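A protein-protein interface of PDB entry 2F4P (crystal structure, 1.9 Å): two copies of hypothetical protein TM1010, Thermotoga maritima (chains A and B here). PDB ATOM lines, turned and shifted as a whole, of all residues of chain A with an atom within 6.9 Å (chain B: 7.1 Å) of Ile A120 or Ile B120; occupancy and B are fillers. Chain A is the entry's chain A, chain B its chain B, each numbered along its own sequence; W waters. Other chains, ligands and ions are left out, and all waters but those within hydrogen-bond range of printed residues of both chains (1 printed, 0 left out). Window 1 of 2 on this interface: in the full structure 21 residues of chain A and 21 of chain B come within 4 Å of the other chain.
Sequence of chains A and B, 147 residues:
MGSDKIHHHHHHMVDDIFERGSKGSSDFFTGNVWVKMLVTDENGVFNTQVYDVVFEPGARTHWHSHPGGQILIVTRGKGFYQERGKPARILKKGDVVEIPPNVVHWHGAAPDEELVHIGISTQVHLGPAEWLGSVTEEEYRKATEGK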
ATOM      1  N   VAL A  39       4.374  13.951 -25.397  1.00  0.00           N
ATOM      2  CA  VAL A  39       5.575  13.150 -25.545  1.00  0.00           C
ATOM      3  C   VAL A  39       5.163  11.722 -25.798  1.00  0.00           C
ATOM      4  O   VAL A  39       4.572  11.081 -24.934  1.00  0.00           O
ATOM      5  CB  VAL A  39       6.460  13.252 -24.301  1.00  0.00           C
ATOM      6  CG1 VAL A  39       7.667  12.276 -24.382  1.00  0.00           C
ATOM      7  CG2 VAL A  39       6.941  14.704 -24.153  1.00  0.00           C
ATOM      8  N   PHE A  46      13.043   8.450 -22.955  1.00  0.00           N
ATOM      9  CA  PHE A  46      12.539   8.940 -21.674  1.00  0.00           C
ATOM     10  C   PHE A  46      11.882   7.869 -20.797  1.00  0.00           C
ATOM     11  O   PHE A  46      11.751   8.068 -19.583  1.00  0.00           O
ATOM     12  CB  PHE A  46      11.562  10.119 -21.912  1.00  0.00           C
ATOM     13  CG  PHE A  46      12.211  11.314 -22.562  1.00  0.00           C
ATOM     14  CD1 PHE A  46      12.924  12.230 -21.823  1.00  0.00           C
ATOM     15  CD2 PHE A  46      12.132  11.494 -23.932  1.00  0.00           C
ATOM     16  CE1 PHE A  46      13.586  13.309 -22.447  1.00  0.00           C
ATOM     17  CE2 PHE A  46      12.755  12.567 -24.545  1.00  0.00           C
ATOM     18  CZ  PHE A  46      13.495  13.479 -23.786  1.00  0.00           C
ATOM     19  N   THR A  48       8.885   7.269 -20.658  1.00  0.00           N
ATOM     20  CA  THR A  48       7.786   8.064 -20.123  1.00  0.00           C
ATOM     21  C   THR A  48       6.968   8.601 -21.297  1.00  0.00           C
ATOM     22  O   THR A  48       7.534   9.035 -22.292  1.00  0.00           O
ATOM     23  CB  THR A  48       8.363   9.283 -19.363  1.00  0.00           C
ATOM     24  OG1 THR A  48       9.340   8.849 -18.421  1.00  0.00           O
ATOM     25  CG2 THR A  48       7.300  10.083 -18.648  1.00  0.00           C
ATOM     26  N   GLN A  49       5.642   8.569 -21.198  1.00  0.00           N
ATOM     27  CA  GLN A  49       4.818   9.267 -22.156  1.00  0.00           C
ATOM     28  C   GLN A  49       4.043  10.345 -21.439  1.00  0.00           C
ATOM     29  O   GLN A  49       3.788  10.233 -20.245  1.00  0.00           O
ATOM     30  CB  GLN A  49       3.898   8.298 -22.851  1.00  0.00           C
ATOM     31  CG  GLN A  49       4.621   7.438 -23.823  1.00  0.00           C
ATOM     32  CD  GLN A  49       3.699   6.489 -24.520  1.00  0.00           C
ATOM     33  OE1 GLN A  49       2.792   5.920 -23.903  1.00  0.00           O
ATOM     34  NE2 GLN A  49       3.913   6.308 -25.817  1.00  0.00           N
ATOM     35  N   VAL A  50       3.730  11.417 -22.164  1.00  0.00           N
ATOM     36  CA  VAL A  50       3.015  12.569 -21.604  1.00  0.00           C
ATOM     37  C   VAL A  50       1.898  12.968 -22.589  1.00  0.00           C
ATOM     38  O   VAL A  50       2.085  12.983 -23.816  1.00  0.00           O
ATOM     39  CB  VAL A  50       3.959  13.773 -21.340  1.00  0.00           C
ATOM     40  CG1 VAL A  50       3.225  14.901 -20.641  1.00  0.00           C
ATOM     41  CG2 VAL A  50       5.174  13.355 -20.520  1.00  0.00           C
ATOM     42  N   TYR A  51       0.728  13.258 -22.035  1.00  0.00           N
ATOM     43  CA  TYR A  51      -0.420  13.628 -22.851  1.00  0.00           C
ATOM     44  C   TYR A  51      -1.252  14.660 -22.128  1.00  0.00           C
ATOM     45  O   TYR A  51      -1.104  14.869 -20.932  1.00  0.00           O
ATOM     46  CB  TYR A  51      -1.255  12.396 -23.218  1.00  0.00           C
ATOM     47  CG  TYR A  51      -1.186  11.357 -22.149  1.00  0.00           C
ATOM     48  CD1 TYR A  51      -0.126  10.446 -22.098  1.00  0.00           C
ATOM     49  CD2 TYR A  51      -2.151  11.308 -21.157  1.00  0.00           C
ATOM     50  CE1 TYR A  51      -0.032   9.524 -21.080  1.00  0.00           C
ATOM     51  CE2 TYR A  51      -2.075  10.374 -20.143  1.00  0.00           C
ATOM     52  CZ  TYR A  51      -1.022   9.490 -20.108  1.00  0.00           C
ATOM     53  OH  TYR A  51      -0.987   8.591 -19.084  1.00  0.00           O
ATOM     54  N   HIS A  66      -1.962   0.801 -15.132  1.00  0.00           N
ATOM     55  CA  HIS A  66      -0.690   0.903 -15.820  1.00  0.00           C
ATOM     56  C   HIS A  66       0.347   0.153 -14.987  1.00  0.00           C
ATOM     57  O   HIS A  66       0.542   0.482 -13.823  1.00  0.00           O
ATOM     58  CB  HIS A  66      -0.243   2.358 -15.888  1.00  0.00           C
ATOM     59  CG  HIS A  66      -0.986   3.169 -16.901  1.00  0.00           C
ATOM     60  ND1 HIS A  66      -0.524   3.333 -18.190  1.00  0.00           N
ATOM     61  CD2 HIS A  66      -2.161   3.826 -16.831  1.00  0.00           C
ATOM     62  CE1 HIS A  66      -1.386   4.068 -18.869  1.00  0.00           C
ATOM     63  NE2 HIS A  66      -2.383   4.386 -18.066  1.00  0.00           N
ATOM     64  N   GLY A  69       2.655   2.768 -13.529  1.00  0.00           N
ATOM     65  CA  GLY A  69       2.107   3.888 -12.772  1.00  0.00           C
ATOM     66  C   GLY A  69       1.761   5.074 -13.680  1.00  0.00           C
ATOM     67  O   GLY A  69       2.026   5.080 -14.919  1.00  0.00           O
ATOM     68  N   GLN A  70       1.152   6.076 -13.065  1.00  0.00           N
ATOM     69  CA  GLN A  70       0.701   7.257 -13.799  1.00  0.00           C
ATOM     70  C   GLN A  70       0.617   8.433 -12.834  1.00  0.00           C
ATOM     71  O   GLN A  70       0.349   8.245 -11.644  1.00  0.00           O
ATOM     72  CB  GLN A  70      -0.669   6.923 -14.458  1.00  0.00           C
ATOM     73  CG  GLN A  70      -1.335   8.051 -15.262  1.00  0.00           C
ATOM     74  CD  GLN A  70      -2.651   7.596 -15.970  1.00  0.00           C
ATOM     75  OE1 GLN A  70      -3.504   6.872 -15.390  1.00  0.00           O
ATOM     76  NE2 GLN A  70      -2.792   7.990 -17.227  1.00  0.00           N
ATOM     77  N   ILE A  71       0.874   9.644 -13.353  1.00  0.00           N
ATOM     78  CA  ILE A  71       0.749  10.881 -12.609  1.00  0.00           C
ATOM     79  C   ILE A  71      -0.228  11.782 -13.380  1.00  0.00           C
ATOM     80  O   ILE A  71      -0.063  11.972 -14.587  1.00  0.00           O
ATOM     81  CB  ILE A  71       2.118  11.588 -12.462  1.00  0.00           C
ATOM     82  CG1 ILE A  71       3.066  10.765 -11.572  1.00  0.00           C
ATOM     83  CG2 ILE A  71       1.949  13.021 -11.875  1.00  0.00           C
ATOM     84  CD1 ILE A  71       4.525  11.101 -11.805  1.00  0.00           C
ATOM     85  N   LEU A  72      -1.237  12.316 -12.700  1.00  0.00           N
ATOM     86  CA  LEU A  72      -2.152  13.290 -13.302  1.00  0.00           C
ATOM     87  C   LEU A  72      -1.908  14.659 -12.687  1.00  0.00           C
ATOM     88  O   LEU A  72      -1.691  14.777 -11.474  1.00  0.00           O
ATOM     89  CB  LEU A  72      -3.614  12.933 -13.050  1.00  0.00           C
ATOM     90  CG  LEU A  72      -4.051  11.487 -13.280  1.00  0.00           C
ATOM     91  CD1 LEU A  72      -5.549  11.386 -13.067  1.00  0.00           C
ATOM     92  CD2 LEU A  72      -3.675  11.017 -14.662  1.00  0.00           C
ATOM     93  N   ILE A  73      -1.948  15.683 -13.538  1.00  0.00           N
ATOM     94  CA  ILE A  73      -1.798  17.063 -13.121  1.00  0.00           C
ATOM     95  C   ILE A  73      -2.964  17.829 -13.708  1.00  0.00           C
ATOM     96  O   ILE A  73      -3.039  17.993 -14.923  1.00  0.00           O
ATOM     97  CB  ILE A  73      -0.479  17.665 -13.628  1.00  0.00           C
ATOM     98  CG1 ILE A  73       0.718  16.832 -13.154  1.00  0.00           C
ATOM     99  CG2 ILE A  73      -0.366  19.090 -13.164  1.00  0.00           C
ATOM    100  CD1 ILE A  73       2.039  17.245 -13.796  1.00  0.00           C
ATOM    101  N   HIS A 117      -6.490  17.739 -17.916  1.00  0.00           N
ATOM    102  CA  HIS A 117      -5.302  17.400 -17.181  1.00  0.00           C
ATOM    103  C   HIS A 117      -4.169  16.922 -18.094  1.00  0.00           C
ATOM    104  O   HIS A 117      -4.409  16.448 -19.214  1.00  0.00           O
ATOM    105  CB  HIS A 117      -5.621  16.365 -16.079  1.00  0.00           C
ATOM    106  CG  HIS A 117      -5.796  14.973 -16.575  1.00  0.00           C
ATOM    107  ND1 HIS A 117      -4.730  14.153 -16.867  1.00  0.00           N
ATOM    108  CD2 HIS A 117      -6.912  14.241 -16.810  1.00  0.00           C
ATOM    109  CE1 HIS A 117      -5.182  12.990 -17.300  1.00  0.00           C
ATOM    110  NE2 HIS A 117      -6.502  13.011 -17.258  1.00  0.00           N
ATOM    111  N   ILE A 118      -2.943  17.087 -17.595  1.00  0.00           N
ATOM    112  CA  ILE A 118      -1.772  16.445 -18.144  1.00  0.00           C
ATOM    113  C   ILE A 118      -1.682  15.066 -17.508  1.00  0.00           C
ATOM    114  O   ILE A 118      -1.973  14.892 -16.313  1.00  0.00           O
ATOM    115  CB  ILE A 118      -0.487  17.272 -17.858  1.00  0.00           C
ATOM    116  CG1 ILE A 118      -0.542  18.622 -18.606  1.00  0.00           C
ATOM    117  CG2 ILE A 118       0.779  16.501 -18.277  1.00  0.00           C
ATOM    118  CD1 ILE A 118       0.281  19.714 -17.975  1.00  0.00           C
ATOM    119  N   GLY A 119      -1.359  14.060 -18.311  1.00  0.00           N
ATOM    120  CA  GLY A 119      -1.092  12.725 -17.785  1.00  0.00           C
ATOM    121  C   GLY A 119       0.324  12.317 -18.111  1.00  0.00           C
ATOM    122  O   GLY A 119       0.812  12.614 -19.209  1.00  0.00           O
ATOM    123  N   ILE A 120       0.991  11.664 -17.152  1.00  0.00           N
ATOM    124  CA  ILE A 120       2.337  11.153 -17.345  1.00  0.00           C
ATOM    125  C   ILE A 120       2.282   9.646 -17.094  1.00  0.00           C
ATOM    126  O   ILE A 120       1.953   9.226 -15.977  1.00  0.00           O
ATOM    127  CB  ILE A 120       3.324  11.802 -16.376  1.00  0.00           C
ATOM    128  CG1 ILE A 120       3.237  13.320 -16.467  1.00  0.00           C
ATOM    129  CG2 ILE A 120       4.741  11.347 -16.663  1.00  0.00           C
ATOM    130  CD1 ILE A 120       3.968  14.064 -15.394  1.00  0.00           C
ATOM    131  N   SER A 121       2.528   8.850 -18.128  1.00  0.00           N
ATOM    132  CA  SER A 121       2.686   7.403 -17.962  1.00  0.00           C
ATOM    133  C   SER A 121       4.177   7.137 -17.674  1.00  0.00           C
ATOM    134  O   SER A 121       5.026   7.324 -18.537  1.00  0.00           O
ATOM    135  CB  SER A 121       2.250   6.644 -19.209  1.00  0.00           C
ATOM    136  OG  SER A 121       0.902   6.875 -19.505  1.00  0.00           O
ATOM    137  N   THR A 122       4.461   6.685 -16.463  1.00  0.00           N
ATOM    138  CA  THR A 122       5.807   6.450 -15.999  1.00  0.00           C
ATOM    139  C   THR A 122       6.201   5.004 -16.262  1.00  0.00           C
ATOM    140  O   THR A 122       5.335   4.110 -16.344  1.00  0.00           O
ATOM    141  CB  THR A 122       5.908   6.782 -14.509  1.00  0.00           C
ATOM    142  OG1 THR A 122       4.879   6.080 -13.779  1.00  0.00           O
ATOM    143  CG2 THR A 122       5.703   8.275 -14.312  1.00  0.00           C
ATOM    144  N   VAL B  39       5.824  16.097  -7.625  1.00  0.00           N
ATOM    145  CA  VAL B  39       6.071  14.695  -7.297  1.00  0.00           C
ATOM    146  C   VAL B  39       7.532  14.536  -6.893  1.00  0.00           C
ATOM    147  O   VAL B  39       8.442  14.684  -7.717  1.00  0.00           O
ATOM    148  CB  VAL B  39       5.718  13.752  -8.463  1.00  0.00           C
ATOM    149  CG1 VAL B  39       6.011  12.292  -8.097  1.00  0.00           C
ATOM    150  CG2 VAL B  39       4.251  13.904  -8.818  1.00  0.00           C
ATOM    151  N   PHE B  46       7.875   5.781  -8.766  1.00  0.00           N
ATOM    152  CA  PHE B  46       7.668   6.193 -10.150  1.00  0.00           C
ATOM    153  C   PHE B  46       8.954   6.330 -10.954  1.00  0.00           C
ATOM    154  O   PHE B  46       8.897   6.362 -12.190  1.00  0.00           O
ATOM    155  CB  PHE B  46       6.863   7.501 -10.176  1.00  0.00           C
ATOM    156  CG  PHE B  46       5.522   7.357  -9.568  1.00  0.00           C
ATOM    157  CD1 PHE B  46       4.477   6.782 -10.305  1.00  0.00           C
ATOM    158  CD2 PHE B  46       5.276   7.772  -8.267  1.00  0.00           C
ATOM    159  CE1 PHE B  46       3.225   6.635  -9.737  1.00  0.00           C
ATOM    160  CE2 PHE B  46       4.020   7.616  -7.691  1.00  0.00           C
ATOM    161  CZ  PHE B  46       2.988   7.055  -8.433  1.00  0.00           C
ATOM    162  N   THR B  48      10.542   8.925 -11.260  1.00  0.00           N
ATOM    163  CA  THR B  48      10.206  10.139 -11.985  1.00  0.00           C
ATOM    164  C   THR B  48       9.907  11.216 -10.923  1.00  0.00           C
ATOM    165  O   THR B  48       9.239  10.953  -9.913  1.00  0.00           O
ATOM    166  CB  THR B  48       8.942   9.922 -12.901  1.00  0.00           C
ATOM    167  OG1 THR B  48       9.074   8.733 -13.670  1.00  0.00           O
ATOM    168  CG2 THR B  48       8.754  11.091 -13.879  1.00  0.00           C
ATOM    169  N   GLN B  49      10.427  12.418 -11.127  1.00  0.00           N
ATOM    170  CA  GLN B  49      10.115  13.531 -10.284  1.00  0.00           C
ATOM    171  C   GLN B  49       9.454  14.576 -11.157  1.00  0.00           C
ATOM    172  O   GLN B  49       9.680  14.615 -12.373  1.00  0.00           O
ATOM    173  CB  GLN B  49      11.381  14.068  -9.613  1.00  0.00           C
ATOM    174  CG  GLN B  49      11.882  13.141  -8.536  1.00  0.00           C
ATOM    175  CD  GLN B  49      13.173  13.590  -7.880  1.00  0.00           C
ATOM    176  OE1 GLN B  49      14.083  14.095  -8.530  1.00  0.00           O
ATOM    177  NE2 GLN B  49      13.262  13.379  -6.581  1.00  0.00           N
ATOM    178  N   VAL B  50       8.612  15.392 -10.538  1.00  0.00           N
ATOM    179  CA  VAL B  50       7.882  16.447 -11.238  1.00  0.00           C
ATOM    180  C   VAL B  50       7.907  17.704 -10.382  1.00  0.00           C
ATOM    181  O   VAL B  50       7.642  17.672  -9.164  1.00  0.00           O
ATOM    182  CB  VAL B  50       6.417  16.083 -11.495  1.00  0.00           C
ATOM    183  CG1 VAL B  50       5.767  17.128 -12.326  1.00  0.00           C
ATOM    184  CG2 VAL B  50       6.287  14.693 -12.173  1.00  0.00           C
ATOM    185  N   TYR B  51       8.194  18.814 -11.053  1.00  0.00           N
ATOM    186  CA  TYR B  51       8.353  20.098 -10.420  1.00  0.00           C
ATOM    187  C   TYR B  51       7.658  21.172 -11.278  1.00  0.00           C
ATOM    188  O   TYR B  51       7.360  20.965 -12.458  1.00  0.00           O
ATOM    189  CB  TYR B  51       9.862  20.397 -10.175  1.00  0.00           C
ATOM    190  CG  TYR B  51      10.715  20.605 -11.418  1.00  0.00           C
ATOM    191  CD1 TYR B  51      10.749  21.828 -12.045  1.00  0.00           C
ATOM    192  CD2 TYR B  51      11.494  19.574 -11.954  1.00  0.00           C
ATOM    193  CE1 TYR B  51      11.520  22.043 -13.190  1.00  0.00           C
ATOM    194  CE2 TYR B  51      12.278  19.779 -13.108  1.00  0.00           C
ATOM    195  CZ  TYR B  51      12.278  21.020 -13.724  1.00  0.00           C
ATOM    196  OH  TYR B  51      13.041  21.271 -14.875  1.00  0.00           O
ATOM    197  N   GLY B  68      19.179  11.095 -16.866  1.00  0.00           N
ATOM    198  CA  GLY B  68      17.862  10.759 -17.436  1.00  0.00           C
ATOM    199  C   GLY B  68      17.297  11.852 -18.339  1.00  0.00           C
ATOM    200  O   GLY B  68      17.650  13.013 -18.223  1.00  0.00           O
ATOM    201  N   GLY B  69      16.411  11.503 -19.264  1.00  0.00           N
ATOM    202  CA  GLY B  69      15.895  12.550 -20.161  1.00  0.00           C
ATOM    203  C   GLY B  69      14.967  13.444 -19.341  1.00  0.00           C
ATOM    204  O   GLY B  69      14.306  12.913 -18.434  1.00  0.00           O
ATOM    205  N   GLN B  70      14.931  14.761 -19.636  1.00  0.00           N
ATOM    206  CA  GLN B  70      13.999  15.716 -19.002  1.00  0.00           C
ATOM    207  C   GLN B  70      12.946  16.226 -19.998  1.00  0.00           C
ATOM    208  O   GLN B  70      13.218  16.332 -21.217  1.00  0.00           O
ATOM    209  CB  GLN B  70      14.697  16.942 -18.449  1.00  0.00           C
ATOM    210  CG  GLN B  70      15.947  16.677 -17.697  1.00  0.00           C
ATOM    211  CD  GLN B  70      15.651  15.995 -16.404  1.00  0.00           C
ATOM    212  OE1 GLN B  70      15.196  16.641 -15.461  1.00  0.00           O
ATOM    213  NE2 GLN B  70      15.884  14.671 -16.343  1.00  0.00           N
ATOM    214  N   ILE B  71      11.755  16.546 -19.466  1.00  0.00           N
ATOM    215  CA  ILE B  71      10.634  17.080 -20.268  1.00  0.00           C
ATOM    216  C   ILE B  71      10.140  18.385 -19.616  1.00  0.00           C
ATOM    217  O   ILE B  71       9.821  18.426 -18.429  1.00  0.00           O
ATOM    218  CB  ILE B  71       9.471  16.054 -20.400  1.00  0.00           C
ATOM    219  CG1 ILE B  71       9.951  14.775 -21.095  1.00  0.00           C
ATOM    220  CG2 ILE B  71       8.272  16.666 -21.155  1.00  0.00           C
ATOM    221  CD1 ILE B  71       9.046  13.587 -20.912  1.00  0.00           C
ATOM    222  N   LEU B  72      10.090  19.459 -20.392  1.00  0.00           N
ATOM    223  CA  LEU B  72       9.533  20.704 -19.913  1.00  0.00           C
ATOM    224  C   LEU B  72       8.232  20.957 -20.643  1.00  0.00           C
ATOM    225  O   LEU B  72       8.138  20.718 -21.852  1.00  0.00           O
ATOM    226  CB  LEU B  72      10.481  21.868 -20.180  1.00  0.00           C
ATOM    227  CG  LEU B  72      11.972  21.717 -19.897  1.00  0.00           C
ATOM    228  CD1 LEU B  72      12.639  23.047 -20.178  1.00  0.00           C
ATOM    229  CD2 LEU B  72      12.224  21.269 -18.489  1.00  0.00           C
ATOM    230  N   ILE B  73       7.233  21.436 -19.900  1.00  0.00           N
ATOM    231  CA  ILE B  73       5.956  21.851 -20.462  1.00  0.00           C
ATOM    232  C   ILE B  73       5.698  23.279 -20.003  1.00  0.00           C
ATOM    233  O   ILE B  73       5.496  23.520 -18.815  1.00  0.00           O
ATOM    234  CB  ILE B  73       4.783  20.966 -19.995  1.00  0.00           C
ATOM    235  CG1 ILE B  73       5.035  19.483 -20.324  1.00  0.00           C
ATOM    236  CG2 ILE B  73       3.500  21.443 -20.639  1.00  0.00           C
ATOM    237  CD1 ILE B  73       4.173  18.535 -19.556  1.00  0.00           C
ATOM    238  N   VAL B  97       9.509  20.742 -24.408  1.00  0.00           N
ATOM    239  CA  VAL B  97      10.929  20.552 -24.640  1.00  0.00           C
ATOM    240  C   VAL B  97      11.357  19.176 -24.147  1.00  0.00           C
ATOM    241  O   VAL B  97      11.219  18.852 -22.957  1.00  0.00           O
ATOM    242  CB  VAL B  97      11.751  21.632 -23.902  1.00  0.00           C
ATOM    243  CG1 VAL B  97      13.225  21.533 -24.261  1.00  0.00           C
ATOM    244  CG2 VAL B  97      11.201  22.987 -24.195  1.00  0.00           C
ATOM    245  N   HIS B 117       7.016  26.874 -16.126  1.00  0.00           N
ATOM    246  CA  HIS B 117       6.873  25.584 -16.744  1.00  0.00           C
ATOM    247  C   HIS B 117       6.862  24.463 -15.734  1.00  0.00           C
ATOM    248  O   HIS B 117       7.441  24.564 -14.646  1.00  0.00           O
ATOM    249  CB  HIS B 117       7.954  25.339 -17.814  1.00  0.00           C
ATOM    250  CG  HIS B 117       9.330  25.066 -17.281  1.00  0.00           C
ATOM    251  ND1 HIS B 117       9.744  23.807 -16.887  1.00  0.00           N
ATOM    252  CD2 HIS B 117      10.412  25.872 -17.152  1.00  0.00           C
ATOM    253  CE1 HIS B 117      11.006  23.864 -16.492  1.00  0.00           C
ATOM    254  NE2 HIS B 117      11.437  25.104 -16.650  1.00  0.00           N
ATOM    255  N   ILE B 118       6.211  23.389 -16.144  1.00  0.00           N
ATOM    256  CA  ILE B 118       6.347  22.099 -15.480  1.00  0.00           C
ATOM    257  C   ILE B 118       7.608  21.394 -15.965  1.00  0.00           C
ATOM    258  O   ILE B 118       7.997  21.506 -17.126  1.00  0.00           O
ATOM    259  CB  ILE B 118       5.104  21.219 -15.769  1.00  0.00           C
ATOM    260  CG1 ILE B 118       3.867  21.884 -15.164  1.00  0.00           C
ATOM    261  CG2 ILE B 118       5.291  19.817 -15.176  1.00  0.00           C
ATOM    262  CD1 ILE B 118       2.538  21.374 -15.719  1.00  0.00           C
ATOM    263  N   GLY B 119       8.266  20.674 -15.071  1.00  0.00           N
ATOM    264  CA  GLY B 119       9.422  19.859 -15.437  1.00  0.00           C
ATOM    265  C   GLY B 119       9.252  18.434 -14.959  1.00  0.00           C
ATOM    266  O   GLY B 119       8.763  18.196 -13.865  1.00  0.00           O
ATOM    267  N   ILE B 120       9.656  17.490 -15.796  1.00  0.00           N
ATOM    268  CA  ILE B 120       9.561  16.073 -15.481  1.00  0.00           C
ATOM    269  C   ILE B 120      10.959  15.508 -15.663  1.00  0.00           C
ATOM    270  O   ILE B 120      11.534  15.590 -16.767  1.00  0.00           O
ATOM    271  CB  ILE B 120       8.612  15.373 -16.448  1.00  0.00           C
ATOM    272  CG1 ILE B 120       7.259  16.100 -16.475  1.00  0.00           C
ATOM    273  CG2 ILE B 120       8.427  13.894 -16.094  1.00  0.00           C
ATOM    274  CD1 ILE B 120       6.319  15.564 -17.553  1.00  0.00           C
ATOM    275  N   SER B 121      11.520  14.984 -14.584  1.00  0.00           N
ATOM    276  CA  SER B 121      12.813  14.300 -14.626  1.00  0.00           C
ATOM    277  C   SER B 121      12.539  12.805 -14.760  1.00  0.00           C
ATOM    278  O   SER B 121      11.893  12.200 -13.893  1.00  0.00           O
ATOM    279  CB  SER B 121      13.600  14.586 -13.347  1.00  0.00           C
ATOM    280  OG  SER B 121      13.839  15.980 -13.224  1.00  0.00           O
ATOM    281  N   THR B 122      12.990  12.202 -15.856  1.00  0.00           N
ATOM    282  CA  THR B 122      12.741  10.773 -16.043  1.00  0.00           C
ATOM    283  C   THR B 122      13.965   9.998 -15.630  1.00  0.00           C
ATOM    284  O   THR B 122      15.088  10.550 -15.540  1.00  0.00           O
ATOM    285  CB  THR B 122      12.370  10.415 -17.510  1.00  0.00           C
ATOM    286  OG1 THR B 122      13.514  10.562 -18.361  1.00  0.00           O
ATOM    287  CG2 THR B 122      11.242  11.333 -18.009  1.00  0.00           C
ATOM    288  N   VAL B 124      15.066   8.723 -12.927  1.00  0.00           N
ATOM    289  CA  VAL B 124      15.748   9.419 -11.848  1.00  0.00           C
ATOM    290  C   VAL B 124      16.911   8.574 -11.286  1.00  0.00           C
ATOM    291  O   VAL B 124      17.977   9.126 -11.014  1.00  0.00           O
ATOM    292  CB  VAL B 124      14.761   9.845 -10.756  1.00  0.00           C
ATOM    293  CG1 VAL B 124      15.483  10.357  -9.531  1.00  0.00           C
ATOM    294  CG2 VAL B 124      13.836  10.916 -11.307  1.00  0.00           C
HETATM  295  O   HOH W   1       8.895   7.240 -16.134  1.00  0.00           O
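Water W1 bridges OG1 of Thr A48 (2.8 Å) and OG1 of Thr B48 (2.9 Å).
Printed residues of chain A that touch a printed residue of chain B: Val A39, Phe A46, Thr A48, Val A50, Gln A70, Ile A71, Ile A118, Ile A120 and Thr A122.
Hydrophobic or aromatic side chains of chain A within 4 Å of the printed part of chain B: Val A39, Phe A46, Val A50, Ile A71, Ile A118 and Ile A120.
Printed residues of chain B that touch a printed residue of chain A: Val B39, Phe B46, Thr B48, Gly B69, Gln B70, Ile B71, Ile B73, Ile B118, Ile B120 and Thr B122.
Hydrophobic or aromatic side chains of chain B within 4 Å of the printed part of chain A: Val B39, Phe B46, Ile B71, Ile B73, Ile B118 and Ile B120.
Among the printed residues, 15 pairs touch across the chains.
Among the printed residues, no Asp or Glu carboxylate lies within 4 Å of a Lys or Arg side-chain nitrogen of the other chain.
CG2 of Ile B71 touches CG2 of Val A39, 3.8 Å away.
Gly B69 touches Phe A46.
Phe A46 touches Gln B70 (CE1 to O, 3.3 Å).
Thr B122 touches Thr A48 (CG2 to OG1, 3.2 Å).
Val A50 touches Ile B120 (CG2 to CD1, 3.9 Å).
Gln A70 touches Phe B46.
CG2 of Val B39 touches CG2 of Ile A71 (3.9 Å).
Ile A120 touches Ile B120.
Thr A122 touches Phe B46 (OG1 to CD1, 3.6 Å).
Thr B48 touches Thr A122 (OG1 to CG2, 3.5 Å).
Phe A46 touches Gln B70, and with the chains exchanged Gln A70 touches Phe B46.
Thr A48 touches Thr B122, and with the chains exchanged Thr A122 touches Thr B48.
Val A50 touches Ile B120, but with the chains exchanged Ile A120 does not touch Val B50 (4.02 Å).
Ile B120 touches its own counterpart, Ile A120.
Of the 15 pairs that touch across the chains among the printed residues, 10 have their exchanged pair printed and touching as well.
OH of Tyr A51 lies within hydrogen-bond range of NE2 of Gln A70 (2.7 Å).
O of Ile B71 lies within hydrogen-bond range of N of Ile B120 (2.8 Å).
O of Val A39 lies within hydrogen-bond range of N of Val A50, at 2.9 Å.
OG1 of Thr B48 lies within hydrogen-bond range of O of Phe B46.
The side-chain hydroxyl of Thr B122 is in hydrogen-bond range of the backbone carbonyl oxygen of Gly B69 (2.5 Å).
The backbone NH (N) of Ile A118 is in hydrogen-bond range of the backbone carbonyl oxygen (O) of Ile A73, at 2.8 Å.
The side-chain hydroxyl (OG1) of Thr B122 sits close to the backbone carbonyl oxygen (O) of Phe A46 (3.3 Å).
Of the printed residues of chain B, Ile A71 touches Val B39.
Of the printed residues of chain B, Ile A120 touches Ile B120 (3.5 Å).
Of the printed residues of chain A, Thr B48 touches Thr A122 (3.5 Å).
Printed residues of chain A within 4 Å of Ile B118: Ile A118.
Ile B120 touches two residues of chain A.
The nearest printed residue of chain B that does not touch Ile A120 is Val B50 (4.02 Å).
The nearest printed residue of chain A that does not touch Ile B71 is Thr A48 (4.5 Å).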
